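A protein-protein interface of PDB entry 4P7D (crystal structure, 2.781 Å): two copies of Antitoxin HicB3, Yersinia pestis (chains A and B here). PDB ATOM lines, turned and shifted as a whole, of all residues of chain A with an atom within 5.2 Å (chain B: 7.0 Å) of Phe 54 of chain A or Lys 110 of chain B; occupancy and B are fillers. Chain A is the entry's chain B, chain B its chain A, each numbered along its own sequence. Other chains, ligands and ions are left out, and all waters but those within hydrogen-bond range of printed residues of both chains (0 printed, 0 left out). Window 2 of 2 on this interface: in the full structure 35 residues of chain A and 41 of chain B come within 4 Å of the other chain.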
ATOM      1  N   LEU A  49      -6.689   4.462 -17.598  1.00  0.00           N
ATOM      2  CA  LEU A  49      -6.169   4.561 -18.961  1.00  0.00           C
ATOM      3  C   LEU A  49      -5.353   3.344 -19.365  1.00  0.00           C
ATOM      4  O   LEU A  49      -5.878   2.236 -19.439  1.00  0.00           O
ATOM      5  CB  LEU A  49      -5.318   5.819 -19.116  1.00  0.00           C
ATOM      6  CG  LEU A  49      -6.146   7.073 -18.870  1.00  0.00           C
ATOM      7  CD1 LEU A  49      -5.252   8.281 -18.703  1.00  0.00           C
ATOM      8  CD2 LEU A  49      -7.077   7.246 -20.037  1.00  0.00           C
ATOM      9  N   MET A  50      -4.056   3.549 -19.572  1.00  0.00           N
ATOM     10  CA  MET A  50      -3.244   2.660 -20.411  1.00  0.00           C
ATOM     11  C   MET A  50      -3.212   1.159 -20.173  1.00  0.00           C
ATOM     12  O   MET A  50      -2.315   0.484 -20.678  1.00  0.00           O
ATOM     13  CB  MET A  50      -1.813   3.139 -20.384  1.00  0.00           C
ATOM     14  CG  MET A  50      -1.172   3.126 -19.033  1.00  0.00           C
ATOM     15  SD  MET A  50       0.232   4.406 -19.310  1.00  0.00           S
ATOM     16  CE  MET A  50      -0.889   6.024 -19.408  1.00  0.00           C
ATOM     17  N   GLU A  52      -5.795   0.502 -21.350  1.00  0.00           N
ATOM     18  CA  GLU A  52      -6.448   0.792 -22.620  1.00  0.00           C
ATOM     19  C   GLU A  52      -5.426   1.211 -23.687  1.00  0.00           C
ATOM     20  O   GLU A  52      -5.786   1.496 -24.828  1.00  0.00           O
ATOM     21  CB  GLU A  52      -7.500   1.896 -22.444  1.00  0.00           C
ATOM     22  CG  GLU A  52      -8.312   1.811 -21.151  1.00  0.00           C
ATOM     23  CD  GLU A  52      -9.366   2.906 -21.019  1.00  0.00           C
ATOM     24  OE1 GLU A  52      -9.249   3.948 -21.699  1.00  0.00           O
ATOM     25  OE2 GLU A  52     -10.308   2.726 -20.215  1.00  0.00           O
ATOM     26  N   GLY A  53      -4.153   1.248 -23.308  1.00  0.00           N
ATOM     27  CA  GLY A  53      -3.091   1.644 -24.217  1.00  0.00           C
ATOM     28  C   GLY A  53      -3.034   3.139 -24.492  1.00  0.00           C
ATOM     29  O   GLY A  53      -2.845   3.564 -25.639  1.00  0.00           O
ATOM     30  N   PHE A  54      -3.189   3.939 -23.440  1.00  0.00           N
ATOM     31  CA  PHE A  54      -3.146   5.395 -23.563  1.00  0.00           C
ATOM     32  C   PHE A  54      -1.788   5.973 -23.137  1.00  0.00           C
ATOM     33  O   PHE A  54      -1.028   5.322 -22.418  1.00  0.00           O
ATOM     34  CB  PHE A  54      -4.281   6.019 -22.760  1.00  0.00           C
ATOM     35  CG  PHE A  54      -5.563   6.106 -23.521  1.00  0.00           C
ATOM     36  CD1 PHE A  54      -5.730   7.066 -24.501  1.00  0.00           C
ATOM     37  CD2 PHE A  54      -6.597   5.225 -23.272  1.00  0.00           C
ATOM     38  CE1 PHE A  54      -6.914   7.153 -25.208  1.00  0.00           C
ATOM     39  CE2 PHE A  54      -7.779   5.307 -23.979  1.00  0.00           C
ATOM     40  CZ  PHE A  54      -7.936   6.273 -24.947  1.00  0.00           C
ATOM     41  N   PRO A  55      -1.460   7.187 -23.611  1.00  0.00           N
ATOM     42  CA  PRO A  55      -0.098   7.660 -23.345  1.00  0.00           C
ATOM     43  C   PRO A  55      -0.014   8.541 -22.101  1.00  0.00           C
ATOM     44  O   PRO A  55      -0.991   9.174 -21.735  1.00  0.00           O
ATOM     45  CB  PRO A  55       0.234   8.462 -24.612  1.00  0.00           C
ATOM     46  CG  PRO A  55      -1.104   9.014 -25.071  1.00  0.00           C
ATOM     47  CD  PRO A  55      -2.177   8.056 -24.569  1.00  0.00           C
ATOM     48  N   LEU A  56       1.144   8.578 -21.461  1.00  0.00           N
ATOM     49  CA  LEU A  56       1.382   9.531 -20.387  1.00  0.00           C
ATOM     50  C   LEU A  56       1.269  10.937 -20.956  1.00  0.00           C
ATOM     51  O   LEU A  56       1.626  11.166 -22.112  1.00  0.00           O
ATOM     52  CB  LEU A  56       2.765   9.330 -19.763  1.00  0.00           C
ATOM     53  CG  LEU A  56       3.169   8.015 -19.089  1.00  0.00           C
ATOM     54  CD1 LEU A  56       4.655   8.087 -18.770  1.00  0.00           C
ATOM     55  CD2 LEU A  56       2.374   7.719 -17.822  1.00  0.00           C
ATOM     56  N   GLU A  90       4.743   2.874 -19.402  1.00  0.00           N
ATOM     57  CA  GLU A  90       4.527   2.494 -20.791  1.00  0.00           C
ATOM     58  C   GLU A  90       5.197   1.153 -21.086  1.00  0.00           C
ATOM     59  O   GLU A  90       6.288   0.847 -20.586  1.00  0.00           O
ATOM     60  CB  GLU A  90       4.994   3.606 -21.750  1.00  0.00           C
ATOM     61  CG  GLU A  90       3.900   4.683 -21.920  1.00  0.00           C
ATOM     62  CD  GLU A  90       4.274   5.893 -22.776  1.00  0.00           C
ATOM     63  OE1 GLU A  90       3.390   6.760 -22.939  1.00  0.00           O
ATOM     64  OE2 GLU A  90       5.412   6.000 -23.285  1.00  0.00           O
ATOM     65  N   ASN B 103       2.366   2.511 -26.355  1.00  0.00           N
ATOM     66  CA  ASN B 103       1.357   3.521 -26.111  1.00  0.00           C
ATOM     67  C   ASN B 103       1.529   4.719 -27.023  1.00  0.00           C
ATOM     68  O   ASN B 103       0.599   5.093 -27.730  1.00  0.00           O
ATOM     69  CB  ASN B 103       1.388   3.951 -24.660  1.00  0.00           C
ATOM     70  CG  ASN B 103       1.168   2.788 -23.709  1.00  0.00           C
ATOM     71  OD1 ASN B 103       2.060   1.947 -23.527  1.00  0.00           O
ATOM     72  ND2 ASN B 103      -0.019   2.727 -23.100  1.00  0.00           N
ATOM     73  N   LEU B 104       2.716   5.304 -27.057  1.00  0.00           N
ATOM     74  CA  LEU B 104       2.907   6.449 -27.934  1.00  0.00           C
ATOM     75  C   LEU B 104       2.619   6.092 -29.416  1.00  0.00           C
ATOM     76  O   LEU B 104       1.917   6.824 -30.129  1.00  0.00           O
ATOM     77  CB  LEU B 104       4.321   7.007 -27.770  1.00  0.00           C
ATOM     78  CG  LEU B 104       4.609   8.357 -28.432  1.00  0.00           C
ATOM     79  CD1 LEU B 104       3.467   9.289 -28.105  1.00  0.00           C
ATOM     80  CD2 LEU B 104       5.947   8.935 -27.972  1.00  0.00           C
ATOM     81  N   LEU B 105       3.130   4.958 -29.880  1.00  0.00           N
ATOM     82  CA  LEU B 105       2.911   4.590 -31.276  1.00  0.00           C
ATOM     83  C   LEU B 105       1.430   4.302 -31.564  1.00  0.00           C
ATOM     84  O   LEU B 105       0.963   4.547 -32.669  1.00  0.00           O
ATOM     85  CB  LEU B 105       3.772   3.384 -31.672  1.00  0.00           C
ATOM     86  CG  LEU B 105       3.825   3.130 -33.184  1.00  0.00           C
ATOM     87  CD1 LEU B 105       4.297   4.353 -33.932  1.00  0.00           C
ATOM     88  CD2 LEU B 105       4.719   1.973 -33.534  1.00  0.00           C
ATOM     89  N   THR B 106       0.682   3.797 -30.582  1.00  0.00           N
ATOM     90  CA  THR B 106      -0.749   3.599 -30.803  1.00  0.00           C
ATOM     91  C   THR B 106      -1.463   4.943 -30.933  1.00  0.00           C
ATOM     92  O   THR B 106      -2.326   5.107 -31.787  1.00  0.00           O
ATOM     93  CB  THR B 106      -1.404   2.804 -29.689  1.00  0.00           C
ATOM     94  OG1 THR B 106      -0.740   1.547 -29.534  1.00  0.00           O
ATOM     95  CG2 THR B 106      -2.816   2.548 -30.043  1.00  0.00           C
ATOM     96  N   ALA B 107      -1.086   5.910 -30.100  1.00  0.00           N
ATOM     97  CA  ALA B 107      -1.725   7.222 -30.123  1.00  0.00           C
ATOM     98  C   ALA B 107      -1.445   7.967 -31.435  1.00  0.00           C
ATOM     99  O   ALA B 107      -2.343   8.566 -32.030  1.00  0.00           O
ATOM    100  CB  ALA B 107      -1.276   8.051 -28.941  1.00  0.00           C
ATOM    101  N   ILE B 108      -0.196   7.925 -31.879  1.00  0.00           N
ATOM    102  CA  ILE B 108       0.162   8.478 -33.181  1.00  0.00           C
ATOM    103  C   ILE B 108      -0.714   7.879 -34.291  1.00  0.00           C
ATOM    104  O   ILE B 108      -1.180   8.589 -35.177  1.00  0.00           O
ATOM    105  CB  ILE B 108       1.652   8.230 -33.491  1.00  0.00           C
ATOM    106  CG1 ILE B 108       2.522   8.992 -32.492  1.00  0.00           C
ATOM    107  CG2 ILE B 108       1.994   8.650 -34.889  1.00  0.00           C
ATOM    108  CD1 ILE B 108       3.982   8.673 -32.601  1.00  0.00           C
ATOM    109  N   ASP B 109      -0.971   6.576 -34.208  1.00  0.00           N
ATOM    110  CA  ASP B 109      -1.890   5.923 -35.125  1.00  0.00           C
ATOM    111  C   ASP B 109      -3.335   6.440 -35.010  1.00  0.00           C
ATOM    112  O   ASP B 109      -3.955   6.798 -36.031  1.00  0.00           O
ATOM    113  CB  ASP B 109      -1.859   4.413 -34.909  1.00  0.00           C
ATOM    114  CG  ASP B 109      -0.509   3.801 -35.260  1.00  0.00           C
ATOM    115  OD1 ASP B 109       0.137   4.289 -36.231  1.00  0.00           O
ATOM    116  OD2 ASP B 109      -0.093   2.835 -34.565  1.00  0.00           O
ATOM    117  N   LYS B 110      -3.878   6.472 -33.787  1.00  0.00           N
ATOM    118  CA  LYS B 110      -5.239   6.981 -33.593  1.00  0.00           C
ATOM    119  C   LYS B 110      -5.358   8.454 -34.021  1.00  0.00           C
ATOM    120  O   LYS B 110      -6.326   8.852 -34.666  1.00  0.00           O
ATOM    121  CB  LYS B 110      -5.684   6.816 -32.146  1.00  0.00           C
ATOM    122  CG  LYS B 110      -6.620   7.901 -31.656  1.00  0.00           C
ATOM    123  CD  LYS B 110      -6.745   7.858 -30.133  1.00  0.00           C
ATOM    124  CE  LYS B 110      -7.376   9.133 -29.574  1.00  0.00           C
ATOM    125  NZ  LYS B 110      -6.967   9.349 -28.161  1.00  0.00           N
ATOM    126  N   PHE B 111      -4.364   9.258 -33.675  1.00  0.00           N
ATOM    127  CA  PHE B 111      -4.366  10.652 -34.079  1.00  0.00           C
ATOM    128  C   PHE B 111      -4.438  10.758 -35.594  1.00  0.00           C
ATOM    129  O   PHE B 111      -5.244  11.503 -36.134  1.00  0.00           O
ATOM    130  CB  PHE B 111      -3.121  11.351 -33.554  1.00  0.00           C
ATOM    131  CG  PHE B 111      -3.162  12.838 -33.668  1.00  0.00           C
ATOM    132  CD1 PHE B 111      -3.804  13.601 -32.708  1.00  0.00           C
ATOM    133  CD2 PHE B 111      -2.532  13.483 -34.716  1.00  0.00           C
ATOM    134  CE1 PHE B 111      -3.828  14.974 -32.796  1.00  0.00           C
ATOM    135  CE2 PHE B 111      -2.558  14.862 -34.816  1.00  0.00           C
ATOM    136  CZ  PHE B 111      -3.198  15.607 -33.853  1.00  0.00           C
ATOM    137  N   ILE B 112      -3.592   9.991 -36.270  1.00  0.00           N
ATOM    138  CA  ILE B 112      -3.460  10.067 -37.721  1.00  0.00           C
ATOM    139  C   ILE B 112      -4.702   9.536 -38.417  1.00  0.00           C
ATOM    140  O   ILE B 112      -5.203  10.163 -39.343  1.00  0.00           O
ATOM    141  CB  ILE B 112      -2.217   9.293 -38.213  1.00  0.00           C
ATOM    142  CG1 ILE B 112      -0.949  10.099 -37.922  1.00  0.00           C
ATOM    143  CG2 ILE B 112      -2.310   8.998 -39.698  1.00  0.00           C
ATOM    144  CD1 ILE B 112       0.330   9.334 -38.154  1.00  0.00           C
ATOM    145  N   ALA B 113      -5.210   8.395 -37.955  1.00  0.00           N
ATOM    146  CA  ALA B 113      -6.418   7.788 -38.526  1.00  0.00           C
ATOM    147  C   ALA B 113      -7.618   8.728 -38.460  1.00  0.00           C
ATOM    148  O   ALA B 113      -8.558   8.627 -39.252  1.00  0.00           O
ATOM    149  CB  ALA B 113      -6.734   6.502 -37.811  1.00  0.00           C
ATOM    150  N   THR B 114      -7.559   9.650 -37.511  1.00  0.00           N
ATOM    151  CA  THR B 114      -8.657  10.547 -37.214  1.00  0.00           C
ATOM    152  C   THR B 114      -8.439  11.926 -37.842  1.00  0.00           C
ATOM    153  O   THR B 114      -9.265  12.375 -38.618  1.00  0.00           O
ATOM    154  CB  THR B 114      -8.850  10.681 -35.675  1.00  0.00           C
ATOM    155  OG1 THR B 114      -9.168   9.398 -35.105  1.00  0.00           O
ATOM    156  CG2 THR B 114      -9.956  11.647 -35.361  1.00  0.00           C
ATOM    157  N   ASN B 115      -7.325  12.584 -37.523  1.00  0.00           N
ATOM    158  CA  ASN B 115      -7.088  13.976 -37.931  1.00  0.00           C
ATOM    159  C   ASN B 115      -6.424  14.098 -39.294  1.00  0.00           C
ATOM    160  O   ASN B 115      -5.680  15.057 -39.516  1.00  0.00           O
ATOM    161  CB  ASN B 115      -6.195  14.708 -36.907  1.00  0.00           C
ATOM    162  CG  ASN B 115      -6.813  14.784 -35.509  1.00  0.00           C
ATOM    163  OD1 ASN B 115      -6.968  13.765 -34.817  1.00  0.00           O
ATOM    164  ND2 ASN B 115      -7.139  16.008 -35.075  1.00  0.00           N
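The side-chain amide nitrogen of Asn 103 of chain B lies within hydrogen-bond range of the backbone carbonyl oxygen of Phe 54 of chain A (2.9 Å).
Of chain B, only Asn 103 (2.9 Å) and Lys 110 (3.7 Å) come within 4 Å of Phe 54 of chain A.
Of the printed residues of chain B, Pro 55 of chain A touches Ala 107 (3.99 Å).
Of the printed residues of chain B, Glu 90 of chain A touches Asn 103 (3.7 Å).
Of the printed residues of chain A, Ala 107 of chain B touches Pro 55.
Lys 110 of chain B touches just one residue of chain A: Phe 54 (3.7 Å).
Ala 113 of chain B touches none of the printed residues of chain A.
The nearest residue of chain B that does not touch Phe 54 of chain A is Leu 104 of chain B (6.0 Å).
The nearest printed residue of chain A that does not touch Asn 103 of chain B is Pro 55 of chain A (4.2 Å).
O of Lys 110 of chain B is in hydrogen-bond range of OG1 of Thr 114 of chain B, at 2.9 Å.
The backbone NH (N) of Leu 56 of chain A lies within hydrogen-bond range of the side-chain carboxylate (OE1) of Glu 90 of chain A, 3.2 Å away.
No position is printed for both chains.
Among the printed residues, merely in contact across the chains: Met 50 of chain A with Asn 103 of chain B (3.3 Å), Gly 53 of chain A with Asn 103 of chain B (3.3 Å), Phe 54 of chain A with Lys 110 of chain B (3.7 Å), Pro 55 of chain A with Ala 107 of chain B (3.99 Å) and Glu 90 of chain A with Asn 103 of chain B (3.7 Å).
Of the 8 printed residues of chain A, 5 touch a printed residue of chain B.
Printed residues of chain A that touch a printed residue of chain B: Met 50, Gly 53, Phe 54, Pro 55 and Glu 90.
Of the 13 printed residues of chain B, 3 touch a printed residue of chain A.
Hydrophobic or aromatic side chains of chain B that line the printed part of chain A: Ala 107.
Among the printed residues, 6 pairs touch across the chains.
Among the printed residues, no Asp or Glu carboxylate lies within 4 Å of a Lys or Arg side-chain nitrogen of the other chain.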
